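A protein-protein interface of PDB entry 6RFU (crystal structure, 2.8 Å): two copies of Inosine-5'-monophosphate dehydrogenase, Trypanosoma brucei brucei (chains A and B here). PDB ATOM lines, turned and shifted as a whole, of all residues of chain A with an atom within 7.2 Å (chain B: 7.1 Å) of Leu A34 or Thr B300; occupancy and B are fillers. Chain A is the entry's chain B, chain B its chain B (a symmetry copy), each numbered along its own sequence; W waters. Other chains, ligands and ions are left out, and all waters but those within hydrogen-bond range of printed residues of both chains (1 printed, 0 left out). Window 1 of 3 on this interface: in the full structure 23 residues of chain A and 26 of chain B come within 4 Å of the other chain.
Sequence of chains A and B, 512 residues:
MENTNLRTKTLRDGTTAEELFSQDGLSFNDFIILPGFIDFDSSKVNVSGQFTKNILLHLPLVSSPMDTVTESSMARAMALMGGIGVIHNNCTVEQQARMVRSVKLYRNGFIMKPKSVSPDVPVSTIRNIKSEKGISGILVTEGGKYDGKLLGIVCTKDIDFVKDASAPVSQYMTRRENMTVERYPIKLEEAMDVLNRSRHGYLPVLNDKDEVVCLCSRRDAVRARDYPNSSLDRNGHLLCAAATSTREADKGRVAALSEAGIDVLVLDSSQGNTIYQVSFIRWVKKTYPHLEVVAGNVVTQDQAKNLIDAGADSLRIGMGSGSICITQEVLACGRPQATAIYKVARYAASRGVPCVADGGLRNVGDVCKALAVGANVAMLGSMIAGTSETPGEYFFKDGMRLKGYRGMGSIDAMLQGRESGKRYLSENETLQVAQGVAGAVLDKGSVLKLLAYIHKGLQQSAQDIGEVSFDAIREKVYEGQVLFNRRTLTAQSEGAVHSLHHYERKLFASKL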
ATOM      1  N   LYS A   9     -24.891  34.156   6.958  1.00  0.00           N
ATOM      2  CA  LYS A   9     -24.435  32.813   7.281  1.00  0.00           C
ATOM      3  C   LYS A   9     -23.525  32.254   6.204  1.00  0.00           C
ATOM      4  O   LYS A   9     -23.811  32.366   5.013  1.00  0.00           O
ATOM      5  CB  LYS A   9     -25.635  31.883   7.482  1.00  0.00           C
ATOM      6  CG  LYS A   9     -26.497  32.267   8.671  1.00  0.00           C
ATOM      7  CD  LYS A   9     -27.719  31.398   8.799  1.00  0.00           C
ATOM      8  CE  LYS A   9     -28.637  31.946   9.881  1.00  0.00           C
ATOM      9  NZ  LYS A   9     -29.857  32.592   9.340  1.00  0.00           N
ATOM     10  N   LEU A  11     -21.488  29.075   7.309  1.00  0.00           N
ATOM     11  CA  LEU A  11     -21.672  27.685   7.718  1.00  0.00           C
ATOM     12  C   LEU A  11     -23.044  27.174   7.292  1.00  0.00           C
ATOM     13  O   LEU A  11     -23.173  26.049   6.807  1.00  0.00           O
ATOM     14  CB  LEU A  11     -21.496  27.548   9.230  1.00  0.00           C
ATOM     15  CG  LEU A  11     -20.079  27.842   9.729  1.00  0.00           C
ATOM     16  CD1 LEU A  11     -20.025  28.056  11.227  1.00  0.00           C
ATOM     17  CD2 LEU A  11     -19.154  26.712   9.336  1.00  0.00           C
ATOM     18  N   ARG A  12     -24.058  28.016   7.469  1.00  0.00           N
ATOM     19  CA  ARG A  12     -25.428  27.695   7.074  1.00  0.00           C
ATOM     20  C   ARG A  12     -25.867  26.349   7.642  1.00  0.00           C
ATOM     21  O   ARG A  12     -26.224  25.432   6.904  1.00  0.00           O
ATOM     22  CB  ARG A  12     -25.564  27.688   5.552  1.00  0.00           C
ATOM     23  CG  ARG A  12     -25.338  29.046   4.882  1.00  0.00           C
ATOM     24  CD  ARG A  12     -25.477  28.913   3.374  1.00  0.00           C
ATOM     25  NE  ARG A  12     -24.438  28.028   2.833  1.00  0.00           N
ATOM     26  CZ  ARG A  12     -23.497  28.382   1.959  1.00  0.00           C
ATOM     27  NH1 ARG A  12     -23.439  29.623   1.468  1.00  0.00           N
ATOM     28  NH2 ARG A  12     -22.610  27.477   1.558  1.00  0.00           N
ATOM     29  N   ASP A  13     -25.814  26.246   8.965  1.00  0.00           N
ATOM     30  CA  ASP A  13     -26.262  25.059   9.677  1.00  0.00           C
ATOM     31  C   ASP A  13     -27.777  25.050   9.809  1.00  0.00           C
ATOM     32  O   ASP A  13     -28.340  25.744  10.659  1.00  0.00           O
ATOM     33  CB  ASP A  13     -25.607  25.002  11.055  1.00  0.00           C
ATOM     34  CG  ASP A  13     -26.209  23.952  11.937  1.00  0.00           C
ATOM     35  OD1 ASP A  13     -26.657  22.916  11.408  1.00  0.00           O
ATOM     36  OD2 ASP A  13     -26.228  24.161  13.164  1.00  0.00           O
ATOM     37  N   GLY A  14     -28.429  24.258   8.961  1.00  0.00           N
ATOM     38  CA  GLY A  14     -29.879  24.180   8.939  1.00  0.00           C
ATOM     39  C   GLY A  14     -30.419  23.808   7.571  1.00  0.00           C
ATOM     40  O   GLY A  14     -29.706  23.873   6.582  1.00  0.00           O
ATOM     41  N   THR A  15     -31.683  23.412   7.519  1.00  0.00           N
ATOM     42  CA  THR A  15     -32.329  23.070   6.259  1.00  0.00           C
ATOM     43  C   THR A  15     -32.853  24.309   5.546  1.00  0.00           C
ATOM     44  O   THR A  15     -33.422  25.209   6.161  1.00  0.00           O
ATOM     45  CB  THR A  15     -33.510  22.106   6.461  1.00  0.00           C
ATOM     46  OG1 THR A  15     -33.157  21.092   7.413  1.00  0.00           O
ATOM     47  CG2 THR A  15     -33.898  21.468   5.135  1.00  0.00           C
ATOM     48  N   ILE A  32     -39.533  24.080  12.713  1.00  0.00           N
ATOM     49  CA  ILE A  32     -39.271  25.309  13.444  1.00  0.00           C
ATOM     50  C   ILE A  32     -38.283  26.146  12.650  1.00  0.00           C
ATOM     51  O   ILE A  32     -37.519  25.608  11.851  1.00  0.00           O
ATOM     52  CB  ILE A  32     -38.714  25.039  14.851  1.00  0.00           C
ATOM     53  CG1 ILE A  32     -37.442  24.206  14.785  1.00  0.00           C
ATOM     54  CG2 ILE A  32     -39.734  24.312  15.686  1.00  0.00           C
ATOM     55  CD1 ILE A  32     -36.177  25.010  14.863  1.00  0.00           C
ATOM     56  N   ILE A  33     -38.314  27.459  12.858  1.00  0.00           N
ATOM     57  CA  ILE A  33     -37.378  28.359  12.198  1.00  0.00           C
ATOM     58  C   ILE A  33     -36.188  28.601  13.110  1.00  0.00           C
ATOM     59  O   ILE A  33     -36.353  28.992  14.266  1.00  0.00           O
ATOM     60  CB  ILE A  33     -38.032  29.698  11.836  1.00  0.00           C
ATOM     61  CG1 ILE A  33     -39.311  29.453  11.028  1.00  0.00           C
ATOM     62  CG2 ILE A  33     -37.050  30.556  11.049  1.00  0.00           C
ATOM     63  CD1 ILE A  33     -40.041  30.706  10.590  1.00  0.00           C
ATOM     64  N   LEU A  34     -34.991  28.352  12.592  1.00  0.00           N
ATOM     65  CA  LEU A  34     -33.770  28.514  13.373  1.00  0.00           C
ATOM     66  C   LEU A  34     -33.445  29.990  13.570  1.00  0.00           C
ATOM     67  O   LEU A  34     -33.677  30.798  12.676  1.00  0.00           O
ATOM     68  CB  LEU A  34     -32.602  27.810  12.688  1.00  0.00           C
ATOM     69  CG  LEU A  34     -32.747  26.293  12.598  1.00  0.00           C
ATOM     70  CD1 LEU A  34     -31.810  25.725  11.546  1.00  0.00           C
ATOM     71  CD2 LEU A  34     -32.469  25.664  13.954  1.00  0.00           C
ATOM     72  N   PRO A  35     -32.895  30.343  14.741  1.00  0.00           N
ATOM     73  CA  PRO A  35     -32.617  31.740  15.077  1.00  0.00           C
ATOM     74  C   PRO A  35     -31.468  32.317  14.267  1.00  0.00           C
ATOM     75  O   PRO A  35     -30.641  31.558  13.756  1.00  0.00           O
ATOM     76  CB  PRO A  35     -32.246  31.667  16.552  1.00  0.00           C
ATOM     77  CG  PRO A  35     -31.624  30.335  16.695  1.00  0.00           C
ATOM     78  CD  PRO A  35     -32.401  29.432  15.785  1.00  0.00           C
ATOM     79  N   GLY A  36     -31.416  33.640  14.159  1.00  0.00           N
ATOM     80  CA  GLY A  36     -30.326  34.303  13.469  1.00  0.00           C
ATOM     81  C   GLY A  36     -29.493  35.173  14.382  1.00  0.00           C
ATOM     82  O   GLY A  36     -29.082  34.737  15.454  1.00  0.00           O
ATOM     83  N   ASP A 464     -36.155  37.085  16.722  1.00  0.00           N
ATOM     84  CA  ASP A 464     -35.476  35.830  16.999  1.00  0.00           C
ATOM     85  C   ASP A 464     -34.793  35.312  15.739  1.00  0.00           C
ATOM     86  O   ASP A 464     -33.677  34.788  15.791  1.00  0.00           O
ATOM     87  CB  ASP A 464     -36.476  34.810  17.534  1.00  0.00           C
ATOM     88  CG  ASP A 464     -35.799  33.659  18.247  1.00  0.00           C
ATOM     89  OD1 ASP A 464     -35.413  33.854  19.425  1.00  0.00           O
ATOM     90  OD2 ASP A 464     -35.654  32.570  17.636  1.00  0.00           O
ATOM     91  N   ILE A 465     -35.471  35.482  14.607  1.00  0.00           N
ATOM     92  CA  ILE A 465     -34.964  35.051  13.310  1.00  0.00           C
ATOM     93  C   ILE A 465     -33.796  35.935  12.903  1.00  0.00           C
ATOM     94  O   ILE A 465     -32.840  35.466  12.290  1.00  0.00           O
ATOM     95  CB  ILE A 465     -36.075  35.090  12.243  1.00  0.00           C
ATOM     96  CG1 ILE A 465     -37.131  34.042  12.577  1.00  0.00           C
ATOM     97  CG2 ILE A 465     -35.518  34.816  10.859  1.00  0.00           C
ATOM     98  CD1 ILE A 465     -38.397  34.159  11.772  1.00  0.00           C
ATOM     99  N   GLY A 466     -33.883  37.217  13.243  1.00  0.00           N
ATOM    100  CA  GLY A 466     -32.761  38.132  13.096  1.00  0.00           C
ATOM    101  C   GLY A 466     -32.831  39.043  11.888  1.00  0.00           C
ATOM    102  O   GLY A 466     -31.789  39.418  11.350  1.00  0.00           O
ATOM    103  N   GLN A 481     -30.834  31.884   3.388  1.00  0.00           N
ATOM    104  CA  GLN A 481     -30.138  32.484   4.519  1.00  0.00           C
ATOM    105  C   GLN A 481     -30.936  32.355   5.818  1.00  0.00           C
ATOM    106  O   GLN A 481     -30.362  32.389   6.905  1.00  0.00           O
ATOM    107  CB  GLN A 481     -29.844  33.952   4.228  1.00  0.00           C
ATOM    108  CG  GLN A 481     -28.521  34.162   3.543  1.00  0.00           C
ATOM    109  CD  GLN A 481     -27.383  33.978   4.499  1.00  0.00           C
ATOM    110  OE1 GLN A 481     -27.356  34.592   5.568  1.00  0.00           O
ATOM    111  NE2 GLN A 481     -26.448  33.105   4.144  1.00  0.00           N
ATOM    112  N   VAL A 482     -32.256  32.229   5.708  1.00  0.00           N
ATOM    113  CA  VAL A 482     -33.078  31.819   6.839  1.00  0.00           C
ATOM    114  C   VAL A 482     -33.365  30.329   6.702  1.00  0.00           C
ATOM    115  O   VAL A 482     -33.840  29.866   5.663  1.00  0.00           O
ATOM    116  CB  VAL A 482     -34.382  32.611   6.917  1.00  0.00           C
ATOM    117  CG1 VAL A 482     -35.282  32.068   8.041  1.00  0.00           C
ATOM    118  CG2 VAL A 482     -34.067  34.085   7.105  1.00  0.00           C
ATOM    119  N   LEU A 483     -33.076  29.588   7.765  1.00  0.00           N
ATOM    120  CA  LEU A 483     -33.039  28.137   7.705  1.00  0.00           C
ATOM    121  C   LEU A 483     -34.020  27.539   8.684  1.00  0.00           C
ATOM    122  O   LEU A 483     -34.425  28.188   9.647  1.00  0.00           O
ATOM    123  CB  LEU A 483     -31.620  27.631   7.990  1.00  0.00           C
ATOM    124  CG  LEU A 483     -30.548  28.185   7.044  1.00  0.00           C
ATOM    125  CD1 LEU A 483     -29.187  27.659   7.391  1.00  0.00           C
ATOM    126  CD2 LEU A 483     -30.881  27.827   5.632  1.00  0.00           C
ATOM    127  N   PHE A 484     -34.386  26.287   8.423  1.00  0.00           N
ATOM    128  CA  PHE A 484     -35.407  25.590   9.184  1.00  0.00           C
ATOM    129  C   PHE A 484     -34.870  24.280   9.726  1.00  0.00           C
ATOM    130  O   PHE A 484     -33.748  23.888   9.427  1.00  0.00           O
ATOM    131  CB  PHE A 484     -36.627  25.332   8.299  1.00  0.00           C
ATOM    132  CG  PHE A 484     -37.171  26.566   7.653  1.00  0.00           C
ATOM    133  CD1 PHE A 484     -36.502  27.164   6.599  1.00  0.00           C
ATOM    134  CD2 PHE A 484     -38.351  27.135   8.100  1.00  0.00           C
ATOM    135  CE1 PHE A 484     -36.995  28.312   6.007  1.00  0.00           C
ATOM    136  CE2 PHE A 484     -38.855  28.275   7.508  1.00  0.00           C
ATOM    137  CZ  PHE A 484     -38.173  28.867   6.458  1.00  0.00           C
ATOM    138  N   ASN A 485     -35.688  23.620  10.539  1.00  0.00           N
ATOM    139  CA  ASN A 485     -35.411  22.276  11.018  1.00  0.00           C
ATOM    140  C   ASN A 485     -36.712  21.523  11.126  1.00  0.00           C
ATOM    141  O   ASN A 485     -37.615  21.953  11.834  1.00  0.00           O
ATOM    142  CB  ASN A 485     -34.708  22.299  12.375  1.00  0.00           C
ATOM    143  CG  ASN A 485     -33.341  21.615  12.352  1.00  0.00           C
ATOM    144  OD1 ASN A 485     -32.659  21.570  11.328  1.00  0.00           O
ATOM    145  ND2 ASN A 485     -32.940  21.084  13.488  1.00  0.00           N
ATOM    146  N   GLN B 271     -31.319  33.715  23.629  1.00  0.00           N
ATOM    147  CA  GLN B 271     -30.603  33.679  22.359  1.00  0.00           C
ATOM    148  C   GLN B 271     -29.421  34.628  22.352  1.00  0.00           C
ATOM    149  O   GLN B 271     -29.585  35.844  22.221  1.00  0.00           O
ATOM    150  CB  GLN B 271     -31.500  34.047  21.209  1.00  0.00           C
ATOM    151  CG  GLN B 271     -30.733  34.152  19.898  1.00  0.00           C
ATOM    152  CD  GLN B 271     -31.616  34.665  18.814  1.00  0.00           C
ATOM    153  OE1 GLN B 271     -32.796  34.934  19.045  1.00  0.00           O
ATOM    154  NE2 GLN B 271     -31.065  34.815  17.619  1.00  0.00           N
ATOM    155  N   ASN B 273     -26.897  35.099  20.244  1.00  0.00           N
ATOM    156  CA  ASN B 273     -26.247  35.574  19.030  1.00  0.00           C
ATOM    157  C   ASN B 273     -26.661  37.014  18.770  1.00  0.00           C
ATOM    158  O   ASN B 273     -27.238  37.335  17.731  1.00  0.00           O
ATOM    159  CB  ASN B 273     -26.582  34.681  17.832  1.00  0.00           C
ATOM    160  CG  ASN B 273     -25.701  34.974  16.622  1.00  0.00           C
ATOM    161  OD1 ASN B 273     -24.552  35.404  16.766  1.00  0.00           O
ATOM    162  ND2 ASN B 273     -26.236  34.748  15.422  1.00  0.00           N
ATOM    163  N   VAL B 298     -27.097  29.148  22.484  1.00  0.00           N
ATOM    164  CA  VAL B 298     -27.142  28.984  21.028  1.00  0.00           C
ATOM    165  C   VAL B 298     -27.674  27.602  20.634  1.00  0.00           C
ATOM    166  O   VAL B 298     -27.699  26.676  21.443  1.00  0.00           O
ATOM    167  CB  VAL B 298     -25.744  29.182  20.386  1.00  0.00           C
ATOM    168  CG1 VAL B 298     -25.153  30.530  20.773  1.00  0.00           C
ATOM    169  CG2 VAL B 298     -24.793  28.068  20.785  1.00  0.00           C
ATOM    170  N   VAL B 299     -28.094  27.463  19.383  1.00  0.00           N
ATOM    171  CA  VAL B 299     -28.527  26.167  18.877  1.00  0.00           C
ATOM    172  C   VAL B 299     -28.018  25.860  17.468  1.00  0.00           C
ATOM    173  O   VAL B 299     -28.224  24.756  16.971  1.00  0.00           O
ATOM    174  CB  VAL B 299     -30.061  26.059  18.876  1.00  0.00           C
ATOM    175  CG1 VAL B 299     -30.562  25.871  20.282  1.00  0.00           C
ATOM    176  CG2 VAL B 299     -30.689  27.280  18.235  1.00  0.00           C
ATOM    177  N   THR B 300     -27.350  26.817  16.828  1.00  0.00           N
ATOM    178  CA  THR B 300     -26.778  26.577  15.504  1.00  0.00           C
ATOM    179  C   THR B 300     -25.294  26.877  15.446  1.00  0.00           C
ATOM    180  O   THR B 300     -24.758  27.646  16.244  1.00  0.00           O
ATOM    181  CB  THR B 300     -27.455  27.427  14.425  1.00  0.00           C
ATOM    182  OG1 THR B 300     -26.974  28.779  14.509  1.00  0.00           O
ATOM    183  CG2 THR B 300     -28.979  27.383  14.583  1.00  0.00           C
ATOM    184  N   GLN B 301     -24.641  26.265  14.467  1.00  0.00           N
ATOM    185  CA  GLN B 301     -23.224  26.481  14.226  1.00  0.00           C
ATOM    186  C   GLN B 301     -22.938  27.939  13.878  1.00  0.00           C
ATOM    187  O   GLN B 301     -21.883  28.470  14.223  1.00  0.00           O
ATOM    188  CB  GLN B 301     -22.737  25.566  13.102  1.00  0.00           C
ATOM    189  CG  GLN B 301     -22.847  24.101  13.432  1.00  0.00           C
ATOM    190  CD  GLN B 301     -22.207  23.222  12.392  1.00  0.00           C
ATOM    191  OE1 GLN B 301     -21.983  23.642  11.252  1.00  0.00           O
ATOM    192  NE2 GLN B 301     -21.894  21.990  12.777  1.00  0.00           N
ATOM    193  N   ASP B 302     -23.880  28.582  13.196  1.00  0.00           N
ATOM    194  CA  ASP B 302     -23.691  29.952  12.758  1.00  0.00           C
ATOM    195  C   ASP B 302     -23.670  30.895  13.939  1.00  0.00           C
ATOM    196  O   ASP B 302     -22.848  31.804  13.980  1.00  0.00           O
ATOM    197  CB  ASP B 302     -24.787  30.355  11.788  1.00  0.00           C
ATOM    198  CG  ASP B 302     -24.801  29.495  10.553  1.00  0.00           C
ATOM    199  OD1 ASP B 302     -24.070  29.822   9.582  1.00  0.00           O
ATOM    200  OD2 ASP B 302     -25.535  28.485  10.565  1.00  0.00           O
ATOM    201  N   GLN B 303     -24.584  30.684  14.885  1.00  0.00           N
ATOM    202  CA  GLN B 303     -24.573  31.416  16.151  1.00  0.00           C
ATOM    203  C   GLN B 303     -23.259  31.187  16.859  1.00  0.00           C
ATOM    204  O   GLN B 303     -22.609  32.120  17.303  1.00  0.00           O
ATOM    205  CB  GLN B 303     -25.699  30.961  17.078  1.00  0.00           C
ATOM    206  CG  GLN B 303     -27.098  31.321  16.670  1.00  0.00           C
ATOM    207  CD  GLN B 303     -28.112  30.696  17.593  1.00  0.00           C
ATOM    208  OE1 GLN B 303     -28.186  29.476  17.698  1.00  0.00           O
ATOM    209  NE2 GLN B 303     -28.889  31.527  18.287  1.00  0.00           N
ATOM    210  N   ALA B 304     -22.888  29.917  16.964  1.00  0.00           N
ATOM    211  CA  ALA B 304     -21.714  29.506  17.716  1.00  0.00           C
ATOM    212  C   ALA B 304     -20.453  30.176  17.198  1.00  0.00           C
ATOM    213  O   ALA B 304     -19.550  30.512  17.965  1.00  0.00           O
ATOM    214  CB  ALA B 304     -21.566  27.998  17.655  1.00  0.00           C
ATOM    215  N   LYS B 305     -20.393  30.368  15.888  1.00  0.00           N
ATOM    216  CA  LYS B 305     -19.221  30.963  15.274  1.00  0.00           C
ATOM    217  C   LYS B 305     -18.988  32.355  15.840  1.00  0.00           C
ATOM    218  O   LYS B 305     -17.884  32.684  16.260  1.00  0.00           O
ATOM    219  CB  LYS B 305     -19.378  31.026  13.759  1.00  0.00           C
ATOM    220  CG  LYS B 305     -18.184  31.636  13.064  1.00  0.00           C
ATOM    221  CD  LYS B 305     -18.403  31.740  11.561  1.00  0.00           C
ATOM    222  CE  LYS B 305     -17.251  32.466  10.879  1.00  0.00           C
ATOM    223  NZ  LYS B 305     -16.950  33.781  11.508  1.00  0.00           N
ATOM    224  N   LEU B 315     -19.807  27.236  25.600  1.00  0.00           N
ATOM    225  CA  LEU B 315     -21.114  27.593  25.048  1.00  0.00           C
ATOM    226  C   LEU B 315     -22.237  26.793  25.690  1.00  0.00           C
ATOM    227  O   LEU B 315     -22.091  25.595  25.917  1.00  0.00           O
ATOM    228  CB  LEU B 315     -21.139  27.362  23.540  1.00  0.00           C
ATOM    229  CG  LEU B 315     -20.111  28.117  22.701  1.00  0.00           C
ATOM    230  CD1 LEU B 315     -20.087  27.549  21.294  1.00  0.00           C
ATOM    231  CD2 LEU B 315     -20.411  29.606  22.671  1.00  0.00           C
ATOM    232  N   ILE B 317     -25.686  25.160  25.034  1.00  0.00           N
ATOM    233  CA  ILE B 317     -26.558  24.738  23.948  1.00  0.00           C
ATOM    234  C   ILE B 317     -27.947  24.408  24.460  1.00  0.00           C
ATOM    235  O   ILE B 317     -28.102  23.560  25.328  1.00  0.00           O
ATOM    236  CB  ILE B 317     -26.018  23.510  23.223  1.00  0.00           C
ATOM    237  CG1 ILE B 317     -24.560  23.726  22.819  1.00  0.00           C
ATOM    238  CG2 ILE B 317     -26.881  23.218  22.003  1.00  0.00           C
ATOM    239  CD1 ILE B 317     -23.885  22.465  22.299  1.00  0.00           C
ATOM    240  N   GLY B 334     -37.943  24.975  20.423  1.00  0.00           N
ATOM    241  CA  GLY B 334     -36.950  25.248  19.398  1.00  0.00           C
ATOM    242  C   GLY B 334     -36.281  24.019  18.825  1.00  0.00           C
ATOM    243  O   GLY B 334     -36.885  22.950  18.745  1.00  0.00           O
ATOM    244  N   ARG B 335     -35.026  24.178  18.419  1.00  0.00           N
ATOM    245  CA  ARG B 335     -34.303  23.107  17.754  1.00  0.00           C
ATOM    246  C   ARG B 335     -34.150  21.904  18.679  1.00  0.00           C
ATOM    247  O   ARG B 335     -33.696  22.063  19.816  1.00  0.00           O
ATOM    248  CB  ARG B 335     -32.925  23.583  17.301  1.00  0.00           C
ATOM    249  CG  ARG B 335     -32.262  22.645  16.300  1.00  0.00           C
ATOM    250  CD  ARG B 335     -30.926  23.174  15.819  1.00  0.00           C
ATOM    251  NE  ARG B 335     -30.472  22.479  14.619  1.00  0.00           N
ATOM    252  CZ  ARG B 335     -29.266  22.623  14.078  1.00  0.00           C
ATOM    253  NH1 ARG B 335     -28.378  23.437  14.632  1.00  0.00           N
ATOM    254  NH2 ARG B 335     -28.944  21.952  12.979  1.00  0.00           N
ATOM    255  N   PRO B 336     -34.524  20.701  18.199  1.00  0.00           N
ATOM    256  CA  PRO B 336     -34.386  19.478  19.000  1.00  0.00           C
ATOM    257  C   PRO B 336     -32.997  19.337  19.621  1.00  0.00           C
ATOM    258  O   PRO B 336     -31.983  19.388  18.923  1.00  0.00           O
ATOM    259  CB  PRO B 336     -34.657  18.374  17.983  1.00  0.00           C
ATOM    260  CG  PRO B 336     -35.572  18.998  17.021  1.00  0.00           C
ATOM    261  CD  PRO B 336     -35.135  20.414  16.889  1.00  0.00           C
ATOM    262  N   ALA B 340     -29.179  19.821  18.052  1.00  0.00           N
ATOM    263  CA  ALA B 340     -28.505  21.047  18.468  1.00  0.00           C
ATOM    264  C   ALA B 340     -27.165  20.759  19.126  1.00  0.00           C
ATOM    265  O   ALA B 340     -26.164  21.387  18.800  1.00  0.00           O
ATOM    266  CB  ALA B 340     -29.374  21.825  19.410  1.00  0.00           C
ATOM    267  N   LYS B 343     -24.568  19.132  16.474  1.00  0.00           N
ATOM    268  CA  LYS B 343     -24.138  20.055  15.434  1.00  0.00           C
ATOM    269  C   LYS B 343     -23.212  21.116  15.985  1.00  0.00           C
ATOM    270  O   LYS B 343     -22.143  21.353  15.445  1.00  0.00           O
ATOM    271  CB  LYS B 343     -25.347  20.724  14.778  1.00  0.00           C
ATOM    272  CG  LYS B 343     -26.185  19.806  13.899  1.00  0.00           C
ATOM    273  CD  LYS B 343     -25.468  19.483  12.614  1.00  0.00           C
ATOM    274  CE  LYS B 343     -26.393  18.848  11.592  1.00  0.00           C
ATOM    275  NZ  LYS B 343     -25.776  18.858  10.244  1.00  0.00           N
ATOM    276  N   VAL B 344     -23.631  21.761  17.064  1.00  0.00           N
ATOM    277  CA  VAL B 344     -22.871  22.867  17.622  1.00  0.00           C
ATOM    278  C   VAL B 344     -21.599  22.370  18.286  1.00  0.00           C
ATOM    279  O   VAL B 344     -20.543  22.969  18.127  1.00  0.00           O
ATOM    280  CB  VAL B 344     -23.700  23.656  18.648  1.00  0.00           C
ATOM    281  CG1 VAL B 344     -22.846  24.717  19.341  1.00  0.00           C
ATOM    282  CG2 VAL B 344     -24.903  24.298  17.972  1.00  0.00           C
ATOM    283  N   TYR B 347     -18.930  21.535  15.802  1.00  0.00           N
ATOM    284  CA  TYR B 347     -18.327  22.729  15.243  1.00  0.00           C
ATOM    285  C   TYR B 347     -17.373  23.343  16.253  1.00  0.00           C
ATOM    286  O   TYR B 347     -16.211  23.596  15.957  1.00  0.00           O
ATOM    287  CB  TYR B 347     -19.367  23.767  14.841  1.00  0.00           C
ATOM    288  CG  TYR B 347     -18.697  25.067  14.471  1.00  0.00           C
ATOM    289  CD1 TYR B 347     -17.935  25.162  13.319  1.00  0.00           C
ATOM    290  CD2 TYR B 347     -18.786  26.185  15.290  1.00  0.00           C
ATOM    291  CE1 TYR B 347     -17.297  26.339  12.972  1.00  0.00           C
ATOM    292  CE2 TYR B 347     -18.147  27.374  14.946  1.00  0.00           C
ATOM    293  CZ  TYR B 347     -17.402  27.437  13.786  1.00  0.00           C
ATOM    294  OH  TYR B 347     -16.758  28.595  13.424  1.00  0.00           O
HETATM  295  O   HOH W   1     -28.495  28.769  11.441  1.00  0.00           O
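The side-chain carboxylate (OD1) of Asp A464 lies close to the side-chain amide oxygen (OE1) of Gln B271 (2.9 Å).
The side-chain carboxylate of Asp A13 is in salt-bridge range of the guanidinium group of Arg B335 (2.7 Å).
The side-chain carboxylate (OD1) of Asp B302 is in hydrogen-bond range of the backbone NH (N) of Arg A12 (2.8 Å).
The side-chain amide nitrogen (NE2) of Gln B271 lies within hydrogen-bond range of the backbone carbonyl oxygen (O) of Gly A36, 2.9 Å away.
OD2 of Asp A13 sits at hydrogen-bond distance from N of Gln B301.
The side-chain amide nitrogen (ND2) of Asn B273 is in hydrogen-bond range of the backbone carbonyl oxygen (O) of Gly A36 (2.8 Å).
The backbone NH (N) of Asp A13 sits at hydrogen-bond distance from the side-chain carboxylate (OD2) of Asp B302 (2.8 Å).
ND2 of Asn A485 sits close to NE of Arg B335 (3.1 Å).
NZ of Lys A9 lies within hydrogen-bond range of O of Gln A481.
The backbone carbonyl oxygen of Leu A483 sits at hydrogen-bond distance from the backbone NH of Leu A34 (3.0 Å).
The side-chain amide oxygen (OE1) of Gln B303 lies within hydrogen-bond range of the backbone NH (N) of Thr B300 (2.9 Å).
N of Gly A36 is in hydrogen-bond range of O of Ile A465 (3.0 Å).
Among the printed residues, merely in contact across the chains: Lys A9 with Asp B302, Leu A11 with Gln B301, Leu A11 with Asp B302, Leu A11 with Lys B305, Leu A11 with Tyr B347, Asp A13 with Thr B300, Asp A13 with Lys B343, Ile A32 with Arg B335, Leu A34 with Thr B300, Leu A34 with Arg B335, Pro A35 with Gln B271, Pro A35 with Val B299 and Pro A35 with Gln B303.
Thr B300 touches just these residues of chain A: Asp A13 and Leu A34.
Of the printed residues of chain A, Lys B305 touches Leu A11.
Of the printed residues of chain A, Val B299 touches Pro A35 (3.5 Å).
Of the printed residues of chain B, Asp A13 touches Thr B300, Gln B301, Asp B302, Arg B335 and Lys B343.
Of the printed residues of chain B, Asn A485 touches Arg B335 (3.1 Å).
Leu A483 touches none of the printed residues of chain B.
The nearest residue of chain B that does not touch Leu A34 is Val B299 (4.9 Å).
The nearest residue of chain A that does not touch Thr B300 is Pro A35 (4.2 Å).
The nearest printed residue of chain B that does not touch Asn A485 is Pro B336 (4.1 Å).
Of the 19 printed residues of chain A, 10 touch a printed residue of chain B.
Of the 19 printed residues of chain B, 11 touch a printed residue of chain A.
Hydrophobic or aromatic side chains of chain B that line the printed part of chain A: Val B299 and Tyr B347.
Among the printed residues, Asp or Glu carboxylates within 4 Å of a Lys or Arg side-chain nitrogen of the other chain: Asp A13 with Arg B335 (2.7 Å).
No position is printed for both chains.
Of the 21 pairs that touch across the chains among the printed residues, none has its exchanged pair printed and touching as well.
Water W1 lies within hydrogen-bond range of OD2 of Asp B302 (3.1 Å), O of Asp A13 (3.1 Å) and OG1 of Thr B300 (3.4 Å).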
